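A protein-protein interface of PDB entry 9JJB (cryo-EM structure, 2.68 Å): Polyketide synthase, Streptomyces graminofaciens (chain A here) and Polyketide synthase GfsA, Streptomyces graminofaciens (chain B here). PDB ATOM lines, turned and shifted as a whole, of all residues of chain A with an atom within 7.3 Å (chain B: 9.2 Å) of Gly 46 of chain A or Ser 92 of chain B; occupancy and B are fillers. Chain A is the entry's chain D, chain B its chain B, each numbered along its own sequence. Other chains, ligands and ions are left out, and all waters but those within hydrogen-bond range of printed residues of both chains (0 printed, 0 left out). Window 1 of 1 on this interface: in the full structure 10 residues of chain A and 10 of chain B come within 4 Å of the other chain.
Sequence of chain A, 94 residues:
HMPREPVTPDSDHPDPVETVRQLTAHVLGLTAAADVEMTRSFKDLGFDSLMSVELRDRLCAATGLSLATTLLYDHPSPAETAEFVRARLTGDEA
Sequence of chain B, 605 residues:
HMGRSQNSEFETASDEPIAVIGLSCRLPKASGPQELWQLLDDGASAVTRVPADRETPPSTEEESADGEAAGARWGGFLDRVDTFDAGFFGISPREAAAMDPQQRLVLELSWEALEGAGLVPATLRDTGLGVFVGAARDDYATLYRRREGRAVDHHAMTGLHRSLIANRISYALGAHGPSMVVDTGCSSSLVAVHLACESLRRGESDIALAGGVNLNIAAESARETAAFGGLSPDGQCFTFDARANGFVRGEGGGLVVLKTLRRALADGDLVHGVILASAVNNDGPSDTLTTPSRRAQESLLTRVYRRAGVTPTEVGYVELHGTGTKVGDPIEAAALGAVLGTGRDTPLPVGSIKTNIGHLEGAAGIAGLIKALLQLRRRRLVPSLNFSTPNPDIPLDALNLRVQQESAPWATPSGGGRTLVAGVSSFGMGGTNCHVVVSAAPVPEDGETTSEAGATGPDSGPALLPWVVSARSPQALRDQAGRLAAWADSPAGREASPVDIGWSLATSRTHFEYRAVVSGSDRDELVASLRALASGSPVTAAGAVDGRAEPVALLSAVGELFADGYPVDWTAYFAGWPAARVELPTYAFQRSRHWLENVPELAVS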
ATOM      1  N   ALA A  25     -17.047 -12.198   4.324  1.00  0.00           N
ATOM      2  CA  ALA A  25     -18.106 -11.305   4.781  1.00  0.00           C
ATOM      3  C   ALA A  25     -19.328 -12.093   5.235  1.00  0.00           C
ATOM      4  O   ALA A  25     -19.988 -11.720   6.213  1.00  0.00           O
ATOM      5  CB  ALA A  25     -18.480 -10.321   3.673  1.00  0.00           C
ATOM      6  N   VAL A  27     -19.258 -15.025   6.579  1.00  0.00           N
ATOM      7  CA  VAL A  27     -18.917 -15.579   7.887  1.00  0.00           C
ATOM      8  C   VAL A  27     -19.174 -14.551   8.982  1.00  0.00           C
ATOM      9  O   VAL A  27     -19.756 -14.864  10.027  1.00  0.00           O
ATOM     10  CB  VAL A  27     -17.457 -16.070   7.894  1.00  0.00           C
ATOM     11  CG1 VAL A  27     -16.870 -16.010   9.297  1.00  0.00           C
ATOM     12  CG2 VAL A  27     -17.370 -17.482   7.333  1.00  0.00           C
ATOM     13  N   LEU A  28     -18.753 -13.303   8.755  1.00  0.00           N
ATOM     14  CA  LEU A  28     -19.027 -12.238   9.713  1.00  0.00           C
ATOM     15  C   LEU A  28     -20.502 -11.860   9.751  1.00  0.00           C
ATOM     16  O   LEU A  28     -20.948 -11.258  10.733  1.00  0.00           O
ATOM     17  CB  LEU A  28     -18.183 -11.006   9.386  1.00  0.00           C
ATOM     18  CG  LEU A  28     -17.446 -10.357  10.560  1.00  0.00           C
ATOM     19  CD1 LEU A  28     -16.630 -11.390  11.321  1.00  0.00           C
ATOM     20  CD2 LEU A  28     -16.560  -9.219  10.075  1.00  0.00           C
ATOM     21  N   GLY A  29     -21.263 -12.202   8.717  1.00  0.00           N
ATOM     22  CA  GLY A  29     -22.674 -11.887   8.663  1.00  0.00           C
ATOM     23  C   GLY A  29     -23.037 -10.621   7.921  1.00  0.00           C
ATOM     24  O   GLY A  29     -24.200 -10.208   7.976  1.00  0.00           O
ATOM     25  N   LEU A  30     -22.087  -9.992   7.234  1.00  0.00           N
ATOM     26  CA  LEU A  30     -22.380  -8.778   6.492  1.00  0.00           C
ATOM     27  C   LEU A  30     -23.196  -9.102   5.240  1.00  0.00           C
ATOM     28  O   LEU A  30     -23.154 -10.212   4.701  1.00  0.00           O
ATOM     29  CB  LEU A  30     -21.087  -8.054   6.115  1.00  0.00           C
ATOM     30  CG  LEU A  30     -20.368  -7.336   7.259  1.00  0.00           C
ATOM     31  CD1 LEU A  30     -18.891  -7.167   6.944  1.00  0.00           C
ATOM     32  CD2 LEU A  30     -21.017  -5.990   7.541  1.00  0.00           C
ATOM     33  N   SER A  41      -6.950  -5.724  11.629  1.00  0.00           N
ATOM     34  CA  SER A  41      -6.600  -7.089  11.984  1.00  0.00           C
ATOM     35  C   SER A  41      -7.860  -7.947  12.105  1.00  0.00           C
ATOM     36  O   SER A  41      -8.986  -7.447  12.185  1.00  0.00           O
ATOM     37  CB  SER A  41      -5.808  -7.117  13.291  1.00  0.00           C
ATOM     38  OG  SER A  41      -6.548  -6.534  14.350  1.00  0.00           O
ATOM     39  N   PHE A  42      -7.653  -9.267  12.107  1.00  0.00           N
ATOM     40  CA  PHE A  42      -8.774 -10.191  12.239  1.00  0.00           C
ATOM     41  C   PHE A  42      -9.478 -10.016  13.579  1.00  0.00           C
ATOM     42  O   PHE A  42     -10.712 -10.049  13.649  1.00  0.00           O
ATOM     43  CB  PHE A  42      -8.291 -11.631  12.069  1.00  0.00           C
ATOM     44  CG  PHE A  42      -8.279 -12.102  10.642  1.00  0.00           C
ATOM     45  CD1 PHE A  42      -9.463 -12.291   9.951  1.00  0.00           C
ATOM     46  CD2 PHE A  42      -7.082 -12.354   9.993  1.00  0.00           C
ATOM     47  CE1 PHE A  42      -9.455 -12.724   8.637  1.00  0.00           C
ATOM     48  CE2 PHE A  42      -7.066 -12.787   8.680  1.00  0.00           C
ATOM     49  CZ  PHE A  42      -8.254 -12.973   8.002  1.00  0.00           C
ATOM     50  N   LYS A  43      -8.708  -9.827  14.653  1.00  0.00           N
ATOM     51  CA  LYS A  43      -9.308  -9.584  15.961  1.00  0.00           C
ATOM     52  C   LYS A  43     -10.103  -8.285  15.967  1.00  0.00           C
ATOM     53  O   LYS A  43     -11.173  -8.204  16.582  1.00  0.00           O
ATOM     54  CB  LYS A  43      -8.224  -9.557  17.039  1.00  0.00           C
ATOM     55  CG  LYS A  43      -8.726  -9.889  18.433  1.00  0.00           C
ATOM     56  CD  LYS A  43      -7.852  -9.252  19.500  1.00  0.00           C
ATOM     57  CE  LYS A  43      -8.642  -8.267  20.346  1.00  0.00           C
ATOM     58  NZ  LYS A  43      -7.944  -7.946  21.622  1.00  0.00           N
ATOM     59  N   ASP A  44      -9.594  -7.253  15.289  1.00  0.00           N
ATOM     60  CA  ASP A  44     -10.305  -5.984  15.187  1.00  0.00           C
ATOM     61  C   ASP A  44     -11.611  -6.097  14.413  1.00  0.00           C
ATOM     62  O   ASP A  44     -12.460  -5.210  14.536  1.00  0.00           O
ATOM     63  CB  ASP A  44      -9.408  -4.931  14.533  1.00  0.00           C
ATOM     64  CG  ASP A  44      -8.626  -4.120  15.547  1.00  0.00           C
ATOM     65  OD1 ASP A  44      -9.001  -4.133  16.737  1.00  0.00           O
ATOM     66  OD2 ASP A  44      -7.634  -3.470  15.152  1.00  0.00           O
ATOM     67  N   LEU A  45     -11.787  -7.150  13.618  1.00  0.00           N
ATOM     68  CA  LEU A  45     -13.029  -7.381  12.893  1.00  0.00           C
ATOM     69  C   LEU A  45     -14.017  -8.238  13.672  1.00  0.00           C
ATOM     70  O   LEU A  45     -15.131  -8.466  13.189  1.00  0.00           O
ATOM     71  CB  LEU A  45     -12.736  -8.035  11.539  1.00  0.00           C
ATOM     72  CG  LEU A  45     -11.956  -7.190  10.529  1.00  0.00           C
ATOM     73  CD1 LEU A  45     -11.827  -7.924   9.203  1.00  0.00           C
ATOM     74  CD2 LEU A  45     -12.621  -5.836  10.334  1.00  0.00           C
ATOM     75  N   GLY A  46     -13.643  -8.716  14.856  1.00  0.00           N
ATOM     76  CA  GLY A  46     -14.527  -9.541  15.656  1.00  0.00           C
ATOM     77  C   GLY A  46     -14.375 -11.022  15.378  1.00  0.00           C
ATOM     78  O   GLY A  46     -15.362 -11.716  15.118  1.00  0.00           O
ATOM     79  N   PHE A  47     -13.141 -11.517  15.428  1.00  0.00           N
ATOM     80  CA  PHE A  47     -12.836 -12.914  15.154  1.00  0.00           C
ATOM     81  C   PHE A  47     -12.292 -13.575  16.413  1.00  0.00           C
ATOM     82  O   PHE A  47     -11.339 -13.072  17.021  1.00  0.00           O
ATOM     83  CB  PHE A  47     -11.820 -13.039  14.015  1.00  0.00           C
ATOM     84  CG  PHE A  47     -12.442 -13.292  12.672  1.00  0.00           C
ATOM     85  CD1 PHE A  47     -12.746 -14.580  12.266  1.00  0.00           C
ATOM     86  CD2 PHE A  47     -12.717 -12.242  11.812  1.00  0.00           C
ATOM     87  CE1 PHE A  47     -13.316 -14.818  11.029  1.00  0.00           C
ATOM     88  CE2 PHE A  47     -13.287 -12.472  10.574  1.00  0.00           C
ATOM     89  CZ  PHE A  47     -13.587 -13.760  10.182  1.00  0.00           C
ATOM     90  N   ASP A  48     -12.894 -14.695  16.800  1.00  0.00           N
ATOM     91  CA  ASP A  48     -12.426 -15.507  17.912  1.00  0.00           C
ATOM     92  C   ASP A  48     -11.938 -16.855  17.383  1.00  0.00           C
ATOM     93  O   ASP A  48     -11.848 -17.076  16.169  1.00  0.00           O
ATOM     94  CB  ASP A  48     -13.527 -15.661  18.965  1.00  0.00           C
ATOM     95  CG  ASP A  48     -14.793 -16.276  18.406  1.00  0.00           C
ATOM     96  OD1 ASP A  48     -14.923 -16.352  17.169  1.00  0.00           O
ATOM     97  OD2 ASP A  48     -15.660 -16.686  19.207  1.00  0.00           O
ATOM     98  N   MET A  51     -14.600 -18.735  15.199  1.00  0.00           N
ATOM     99  CA  MET A  51     -14.714 -18.120  13.882  1.00  0.00           C
ATOM    100  C   MET A  51     -13.452 -18.314  13.055  1.00  0.00           C
ATOM    101  O   MET A  51     -13.543 -18.484  11.836  1.00  0.00           O
ATOM    102  CB  MET A  51     -15.036 -16.631  14.012  1.00  0.00           C
ATOM    103  CG  MET A  51     -16.480 -16.339  14.386  1.00  0.00           C
ATOM    104  SD  MET A  51     -16.801 -14.579  14.604  1.00  0.00           S
ATOM    105  CE  MET A  51     -17.606 -14.577  16.203  1.00  0.00           C
ATOM    106  N   PHE B  84     -27.008  -0.213  16.570  1.00  0.00           N
ATOM    107  CA  PHE B  84     -25.693  -0.246  17.192  1.00  0.00           C
ATOM    108  C   PHE B  84     -24.623  -0.069  16.124  1.00  0.00           C
ATOM    109  O   PHE B  84     -24.801  -0.475  14.973  1.00  0.00           O
ATOM    110  CB  PHE B  84     -25.470  -1.557  17.955  1.00  0.00           C
ATOM    111  CG  PHE B  84     -24.160  -1.622  18.686  1.00  0.00           C
ATOM    112  CD1 PHE B  84     -23.713  -0.546  19.434  1.00  0.00           C
ATOM    113  CD2 PHE B  84     -23.374  -2.761  18.624  1.00  0.00           C
ATOM    114  CE1 PHE B  84     -22.506  -0.602  20.104  1.00  0.00           C
ATOM    115  CE2 PHE B  84     -22.167  -2.825  19.294  1.00  0.00           C
ATOM    116  CZ  PHE B  84     -21.733  -1.744  20.036  1.00  0.00           C
ATOM    117  N   ASP B  85     -23.510   0.546  16.521  1.00  0.00           N
ATOM    118  CA  ASP B  85     -22.336   0.701  15.663  1.00  0.00           C
ATOM    119  C   ASP B  85     -21.386  -0.444  15.998  1.00  0.00           C
ATOM    120  O   ASP B  85     -20.487  -0.310  16.830  1.00  0.00           O
ATOM    121  CB  ASP B  85     -21.685   2.064  15.872  1.00  0.00           C
ATOM    122  CG  ASP B  85     -20.727   2.435  14.753  1.00  0.00           C
ATOM    123  OD1 ASP B  85     -19.967   1.555  14.295  1.00  0.00           O
ATOM    124  OD2 ASP B  85     -20.731   3.611  14.334  1.00  0.00           O
ATOM    125  N   ALA B  86     -21.594  -1.587  15.340  1.00  0.00           N
ATOM    126  CA  ALA B  86     -20.790  -2.769  15.630  1.00  0.00           C
ATOM    127  C   ALA B  86     -19.344  -2.599  15.183  1.00  0.00           C
ATOM    128  O   ALA B  86     -18.429  -3.098  15.850  1.00  0.00           O
ATOM    129  CB  ALA B  86     -21.409  -3.999  14.967  1.00  0.00           C
ATOM    130  N   GLY B  87     -19.115  -1.908  14.065  1.00  0.00           N
ATOM    131  CA  GLY B  87     -17.766  -1.756  13.548  1.00  0.00           C
ATOM    132  C   GLY B  87     -16.872  -0.865  14.384  1.00  0.00           C
ATOM    133  O   GLY B  87     -15.646  -1.012  14.329  1.00  0.00           O
ATOM    134  N   PHE B  88     -17.454   0.058  15.153  1.00  0.00           N
ATOM    135  CA  PHE B  88     -16.643   0.957  15.970  1.00  0.00           C
ATOM    136  C   PHE B  88     -15.916   0.204  17.077  1.00  0.00           C
ATOM    137  O   PHE B  88     -14.751   0.496  17.372  1.00  0.00           O
ATOM    138  CB  PHE B  88     -17.517   2.066  16.557  1.00  0.00           C
ATOM    139  CG  PHE B  88     -16.739   3.142  17.257  1.00  0.00           C
ATOM    140  CD1 PHE B  88     -16.149   4.169  16.539  1.00  0.00           C
ATOM    141  CD2 PHE B  88     -16.598   3.129  18.636  1.00  0.00           C
ATOM    142  CE1 PHE B  88     -15.433   5.161  17.181  1.00  0.00           C
ATOM    143  CE2 PHE B  88     -15.882   4.118  19.284  1.00  0.00           C
ATOM    144  CZ  PHE B  88     -15.300   5.135  18.555  1.00  0.00           C
ATOM    145  N   PHE B  89     -16.583  -0.764  17.702  1.00  0.00           N
ATOM    146  CA  PHE B  89     -16.015  -1.523  18.806  1.00  0.00           C
ATOM    147  C   PHE B  89     -15.414  -2.851  18.363  1.00  0.00           C
ATOM    148  O   PHE B  89     -15.031  -3.660  19.213  1.00  0.00           O
ATOM    149  CB  PHE B  89     -17.075  -1.762  19.882  1.00  0.00           C
ATOM    150  CG  PHE B  89     -17.645  -0.499  20.463  1.00  0.00           C
ATOM    151  CD1 PHE B  89     -16.996   0.158  21.495  1.00  0.00           C
ATOM    152  CD2 PHE B  89     -18.825   0.035  19.973  1.00  0.00           C
ATOM    153  CE1 PHE B  89     -17.516   1.321  22.031  1.00  0.00           C
ATOM    154  CE2 PHE B  89     -19.350   1.198  20.504  1.00  0.00           C
ATOM    155  CZ  PHE B  89     -18.694   1.842  21.535  1.00  0.00           C
ATOM    156  N   GLY B  90     -15.318  -3.090  17.057  1.00  0.00           N
ATOM    157  CA  GLY B  90     -14.754  -4.327  16.554  1.00  0.00           C
ATOM    158  C   GLY B  90     -15.573  -5.551  16.908  1.00  0.00           C
ATOM    159  O   GLY B  90     -15.026  -6.571  17.337  1.00  0.00           O
ATOM    160  N   ILE B  91     -16.888  -5.459  16.732  1.00  0.00           N
ATOM    161  CA  ILE B  91     -17.812  -6.537  17.059  1.00  0.00           C
ATOM    162  C   ILE B  91     -18.479  -7.001  15.772  1.00  0.00           C
ATOM    163  O   ILE B  91     -18.985  -6.181  14.998  1.00  0.00           O
ATOM    164  CB  ILE B  91     -18.863  -6.088  18.090  1.00  0.00           C
ATOM    165  CG1 ILE B  91     -18.199  -5.815  19.441  1.00  0.00           C
ATOM    166  CG2 ILE B  91     -19.956  -7.136  18.231  1.00  0.00           C
ATOM    167  CD1 ILE B  91     -19.050  -4.998  20.387  1.00  0.00           C
ATOM    168  N   SER B  92     -18.472  -8.313  15.544  1.00  0.00           N
ATOM    169  CA  SER B  92     -19.109  -8.867  14.362  1.00  0.00           C
ATOM    170  C   SER B  92     -20.622  -8.665  14.431  1.00  0.00           C
ATOM    171  O   SER B  92     -21.209  -8.672  15.517  1.00  0.00           O
ATOM    172  CB  SER B  92     -18.786 -10.353  14.229  1.00  0.00           C
ATOM    173  OG  SER B  92     -19.706 -11.003  13.369  1.00  0.00           O
ATOM    174  N   PRO B  93     -21.275  -8.464  13.282  1.00  0.00           N
ATOM    175  CA  PRO B  93     -22.738  -8.287  13.298  1.00  0.00           C
ATOM    176  C   PRO B  93     -23.484  -9.459  13.913  1.00  0.00           C
ATOM    177  O   PRO B  93     -24.496  -9.253  14.593  1.00  0.00           O
ATOM    178  CB  PRO B  93     -23.082  -8.108  11.813  1.00  0.00           C
ATOM    179  CG  PRO B  93     -21.827  -7.582  11.198  1.00  0.00           C
ATOM    180  CD  PRO B  93     -20.703  -8.243  11.942  1.00  0.00           C
ATOM    181  N   ARG B  94     -23.012 -10.689  13.691  1.00  0.00           N
ATOM    182  CA  ARG B  94     -23.660 -11.849  14.295  1.00  0.00           C
ATOM    183  C   ARG B  94     -23.573 -11.799  15.815  1.00  0.00           C
ATOM    184  O   ARG B  94     -24.549 -12.102  16.512  1.00  0.00           O
ATOM    185  CB  ARG B  94     -23.035 -13.138  13.763  1.00  0.00           C
ATOM    186  CG  ARG B  94     -24.008 -14.039  13.018  1.00  0.00           C
ATOM    187  CD  ARG B  94     -24.062 -13.693  11.539  1.00  0.00           C
ATOM    188  NE  ARG B  94     -24.853 -14.655  10.781  1.00  0.00           N
ATOM    189  CZ  ARG B  94     -24.412 -15.841  10.384  1.00  0.00           C
ATOM    190  NH1 ARG B  94     -23.183 -16.248  10.654  1.00  0.00           N
ATOM    191  NH2 ARG B  94     -25.226 -16.639   9.698  1.00  0.00           N
ATOM    192  N   GLU B  95     -22.407 -11.428  16.350  1.00  0.00           N
ATOM    193  CA  GLU B  95     -22.258 -11.311  17.797  1.00  0.00           C
ATOM    194  C   GLU B  95     -23.133 -10.196  18.357  1.00  0.00           C
ATOM    195  O   GLU B  95     -23.754 -10.357  19.414  1.00  0.00           O
ATOM    196  CB  GLU B  95     -20.789 -11.075  18.153  1.00  0.00           C
ATOM    197  CG  GLU B  95     -20.557 -10.601  19.578  1.00  0.00           C
ATOM    198  CD  GLU B  95     -19.086 -10.412  19.895  1.00  0.00           C
ATOM    199  OE1 GLU B  95     -18.312 -10.096  18.967  1.00  0.00           O
ATOM    200  OE2 GLU B  95     -18.704 -10.578  21.073  1.00  0.00           O
ATOM    201  N   ALA B  96     -23.200  -9.059  17.658  1.00  0.00           N
ATOM    202  CA  ALA B  96     -23.999  -7.939  18.143  1.00  0.00           C
ATOM    203  C   ALA B  96     -25.493  -8.218  18.038  1.00  0.00           C
ATOM    204  O   ALA B  96     -26.285  -7.621  18.776  1.00  0.00           O
ATOM    205  CB  ALA B  96     -23.643  -6.667  17.373  1.00  0.00           C
ATOM    206  N   ALA B  97     -25.897  -9.109  17.128  1.00  0.00           N
ATOM    207  CA  ALA B  97     -27.313  -9.427  16.982  1.00  0.00           C
ATOM    208  C   ALA B  97     -27.881 -10.083  18.234  1.00  0.00           C
ATOM    209  O   ALA B  97     -29.000  -9.760  18.647  1.00  0.00           O
ATOM    210  CB  ALA B  97     -27.526 -10.330  15.766  1.00  0.00           C
ATOM    211  N   ALA B  98     -27.134 -10.997  18.847  1.00  0.00           N
ATOM    212  CA  ALA B  98     -27.571 -11.683  20.054  1.00  0.00           C
ATOM    213  C   ALA B  98     -27.106 -10.989  21.329  1.00  0.00           C
ATOM    214  O   ALA B  98     -27.396 -11.477  22.426  1.00  0.00           O
ATOM    215  CB  ALA B  98     -27.081 -13.134  20.044  1.00  0.00           C
ATOM    216  N   MET B  99     -26.398  -9.871  21.211  1.00  0.00           N
ATOM    217  CA  MET B  99     -25.897  -9.149  22.369  1.00  0.00           C
ATOM    218  C   MET B  99     -26.994  -8.293  22.989  1.00  0.00           C
ATOM    219  O   MET B  99     -27.874  -7.776  22.298  1.00  0.00           O
ATOM    220  CB  MET B  99     -24.708  -8.267  21.987  1.00  0.00           C
ATOM    221  CG  MET B  99     -23.818  -7.886  23.159  1.00  0.00           C
ATOM    222  SD  MET B  99     -22.708  -6.520  22.774  1.00  0.00           S
ATOM    223  CE  MET B  99     -21.903  -7.152  21.306  1.00  0.00           C
ATOM    224  N   ARG B 104     -24.347  -2.576  24.806  1.00  0.00           N
ATOM    225  CA  ARG B 104     -23.970  -1.606  23.783  1.00  0.00           C
ATOM    226  C   ARG B 104     -24.198  -0.180  24.271  1.00  0.00           C
ATOM    227  O   ARG B 104     -23.363   0.707  24.051  1.00  0.00           O
ATOM    228  CB  ARG B 104     -24.763  -1.873  22.504  1.00  0.00           C
ATOM    229  CG  ARG B 104     -25.258  -3.306  22.376  1.00  0.00           C
ATOM    230  CD  ARG B 104     -25.868  -3.567  21.010  1.00  0.00           C
ATOM    231  NE  ARG B 104     -26.733  -4.742  21.013  1.00  0.00           N
ATOM    232  CZ  ARG B 104     -27.740  -4.933  20.171  1.00  0.00           C
ATOM    233  NH1 ARG B 104     -28.042  -4.042  19.241  1.00  0.00           N
ATOM    234  NH2 ARG B 104     -28.463  -6.045  20.267  1.00  0.00           N
ATOM    235  N   ASP B 153     -26.189 -20.896  19.766  1.00  0.00           N
ATOM    236  CA  ASP B 153     -24.977 -20.095  19.439  1.00  0.00           C
ATOM    237  C   ASP B 153     -24.000 -20.141  20.616  1.00  0.00           C
ATOM    238  O   ASP B 153     -24.352 -20.728  21.658  1.00  0.00           O
ATOM    239  CB  ASP B 153     -25.349 -18.667  19.073  1.00  0.00           C
ATOM    240  CG  ASP B 153     -24.317 -17.898  18.262  1.00  0.00           C
ATOM    241  OD1 ASP B 153     -23.485 -18.554  17.602  1.00  0.00           O
ATOM    242  OD2 ASP B 153     -24.355 -16.650  18.301  1.00  0.00           O
ATOM    243  N   HIS B 154     -22.821 -19.543  20.457  1.00  0.00           N
ATOM    244  CA  HIS B 154     -21.832 -19.484  21.564  1.00  0.00           C
ATOM    245  C   HIS B 154     -21.767 -18.047  22.082  1.00  0.00           C
ATOM    246  O   HIS B 154     -21.077 -17.797  23.090  1.00  0.00           O
ATOM    247  CB  HIS B 154     -20.472 -20.000  21.084  1.00  0.00           C
ATOM    248  CG  HIS B 154     -19.792 -19.153  20.062  1.00  0.00           C
ATOM    249  ND1 HIS B 154     -20.064 -19.241  18.715  1.00  0.00           N
ATOM    250  CD2 HIS B 154     -18.831 -18.229  20.187  1.00  0.00           C
ATOM    251  CE1 HIS B 154     -19.296 -18.384  18.058  1.00  0.00           C
ATOM    252  NE2 HIS B 154     -18.538 -17.760  18.933  1.00  0.00           N
ATOM    253  N   HIS B 155     -22.461 -17.130  21.403  1.00  0.00           N
ATOM    254  CA  HIS B 155     -22.486 -15.707  21.822  1.00  0.00           C
ATOM    255  C   HIS B 155     -23.651 -15.497  22.780  1.00  0.00           C
ATOM    256  O   HIS B 155     -23.645 -14.501  23.521  1.00  0.00           O
ATOM    257  CB  HIS B 155     -22.681 -14.799  20.613  1.00  0.00           C
ATOM    258  CG  HIS B 155     -21.566 -14.855  19.632  1.00  0.00           C
ATOM    259  ND1 HIS B 155     -21.757 -15.182  18.309  1.00  0.00           N
ATOM    260  CD2 HIS B 155     -20.262 -14.620  19.779  1.00  0.00           C
ATOM    261  CE1 HIS B 155     -20.593 -15.143  17.685  1.00  0.00           C
ATOM    262  NE2 HIS B 155     -19.673 -14.804  18.560  1.00  0.00           N
ATOM    263  N   ARG B 168     -17.076  -6.271  29.555  1.00  0.00           N
ATOM    264  CA  ARG B 168     -16.783  -5.901  28.174  1.00  0.00           C
ATOM    265  C   ARG B 168     -16.054  -4.566  28.106  1.00  0.00           C
ATOM    266  O   ARG B 168     -15.142  -4.390  27.288  1.00  0.00           O
ATOM    267  CB  ARG B 168     -18.077  -5.847  27.359  1.00  0.00           C
ATOM    268  CG  ARG B 168     -17.900  -6.180  25.887  1.00  0.00           C
ATOM    269  CD  ARG B 168     -19.239  -6.223  25.168  1.00  0.00           C
ATOM    270  NE  ARG B 168     -19.935  -7.486  25.381  1.00  0.00           N
ATOM    271  CZ  ARG B 168     -19.697  -8.597  24.698  1.00  0.00           C
ATOM    272  NH1 ARG B 168     -18.782  -8.641  23.744  1.00  0.00           N
ATOM    273  NH2 ARG B 168     -20.394  -9.694  24.980  1.00  0.00           N
ATOM    274  N   TYR B 171     -12.680  -5.102  28.696  1.00  0.00           N
ATOM    275  CA  TYR B 171     -12.101  -5.691  27.495  1.00  0.00           C
ATOM    276  C   TYR B 171     -11.872  -4.631  26.424  1.00  0.00           C
ATOM    277  O   TYR B 171     -10.893  -4.701  25.672  1.00  0.00           O
ATOM    278  CB  TYR B 171     -13.007  -6.804  26.971  1.00  0.00           C
ATOM    279  CG  TYR B 171     -12.524  -7.448  25.691  1.00  0.00           C
ATOM    280  CD1 TYR B 171     -11.344  -8.179  25.661  1.00  0.00           C
ATOM    281  CD2 TYR B 171     -13.252  -7.329  24.515  1.00  0.00           C
ATOM    282  CE1 TYR B 171     -10.901  -8.772  24.494  1.00  0.00           C
ATOM    283  CE2 TYR B 171     -12.817  -7.917  23.343  1.00  0.00           C
ATOM    284  CZ  TYR B 171     -11.641  -8.637  23.338  1.00  0.00           C
ATOM    285  OH  TYR B 171     -11.204  -9.225  22.174  1.00  0.00           O
ATOM    286  N   HIS B 594     -29.756  -4.225  14.664  1.00  0.00           N
ATOM    287  CA  HIS B 594     -29.277  -5.518  15.137  1.00  0.00           C
ATOM    288  C   HIS B 594     -30.305  -6.084  16.103  1.00  0.00           C
ATOM    289  O   HIS B 594     -30.504  -5.534  17.191  1.00  0.00           O
ATOM    290  CB  HIS B 594     -27.910  -5.392  15.818  1.00  0.00           C
ATOM    291  CG  HIS B 594     -26.786  -5.109  14.872  1.00  0.00           C
ATOM    292  ND1 HIS B 594     -25.909  -4.060  15.049  1.00  0.00           N
ATOM    293  CD2 HIS B 594     -26.393  -5.739  13.739  1.00  0.00           C
ATOM    294  CE1 HIS B 594     -25.027  -4.055  14.067  1.00  0.00           C
ATOM    295  NE2 HIS B 594     -25.298  -5.064  13.258  1.00  0.00           N
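The backbone carbonyl oxygen (O) of Leu 28 of chain A sits at hydrogen-bond distance from the side-chain hydroxyl (OG) of Ser 92 of chain B (2.9 Å).
NE2 of His 154 of chain B is in hydrogen-bond range of OD2 of Asp 48 of chain A, 3.1 Å away.
Among the printed residues, merely in contact across the chains: Val 27 of chain A with Arg 94 of chain B (3.7 Å), Leu 28 of chain A with Pro 93 of chain B (3.3 Å), Leu 28 of chain A with Arg 94 of chain B (3.7 Å), Gly 29 of chain A with Arg 94 of chain B (3.7 Å), Lys 43 of chain A with Tyr 171 of chain B (3.3 Å), Asp 44 of chain A with Gly 90 of chain B (3.2 Å), Gly 46 of chain A with Gly 90 of chain B (3.4 Å), Gly 46 of chain A with Ser 92 of chain B (3.8 Å) and Met 51 of chain A with His 155 of chain B (3.1 Å).
Printed residues of chain B within 4 Å of Leu 28 of chain A: Ser 92 (2.9 Å), Pro 93 (3.3 Å) and Arg 94 (3.7 Å).
Of the printed residues of chain B, Gly 29 of chain A touches Arg 94.
Of the printed residues of chain B, Lys 43 of chain A touches Tyr 171.
Of chain B, only Gly 90 and Ser 92 come within 4 Å of Gly 46 of chain A.
Of the printed residues of chain A, Gly 90 of chain B touches Asp 44 (3.2 Å) and Gly 46 (3.4 Å).
Of chain A, only Leu 28 (2.9 Å) and Gly 46 (3.8 Å) come within 4 Å of Ser 92 of chain B.
Printed residues of chain A within 4 Å of Pro 93 of chain B: Leu 28.
The nearest residue of chain A that does not touch Ser 92 of chain B is Leu 45 of chain A (4.1 Å).
The nearest printed residue of chain B that does not touch Leu 28 of chain A is Glu 95 of chain B (5.8 Å).
OG of Ser 92 of chain B sits close to N of Arg 94 of chain B, at 3.3 Å.
The side-chain carboxylate of Asp 153 of chain B is in hydrogen-bond range of a ring nitrogen (ND1) of His 155 of chain B (3.0 Å).
NE2 of His 154 of chain B lies within hydrogen-bond range of NE2 of His 155 of chain B (3.2 Å).
The side-chain hydroxyl (OG) of Ser 41 of chain A lies within hydrogen-bond range of the backbone NH (N) of Asp 44 of chain A.
The backbone NH (N) of Met 51 of chain A sits at hydrogen-bond distance from the side-chain carboxylate (OD1) of Asp 48 of chain A (3.1 Å).
Hydrophobic or aromatic side chains of chain A that line the printed part of chain B: Leu 28 and Met 51.
Hydrophobic or aromatic side chains of chain B that line the printed part of chain A: Pro 93, His 154, His 155 and Tyr 171.
Among the printed residues, no Asp or Glu carboxylate lies within 4 Å of a Lys or Arg side-chain nitrogen of the other chain.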
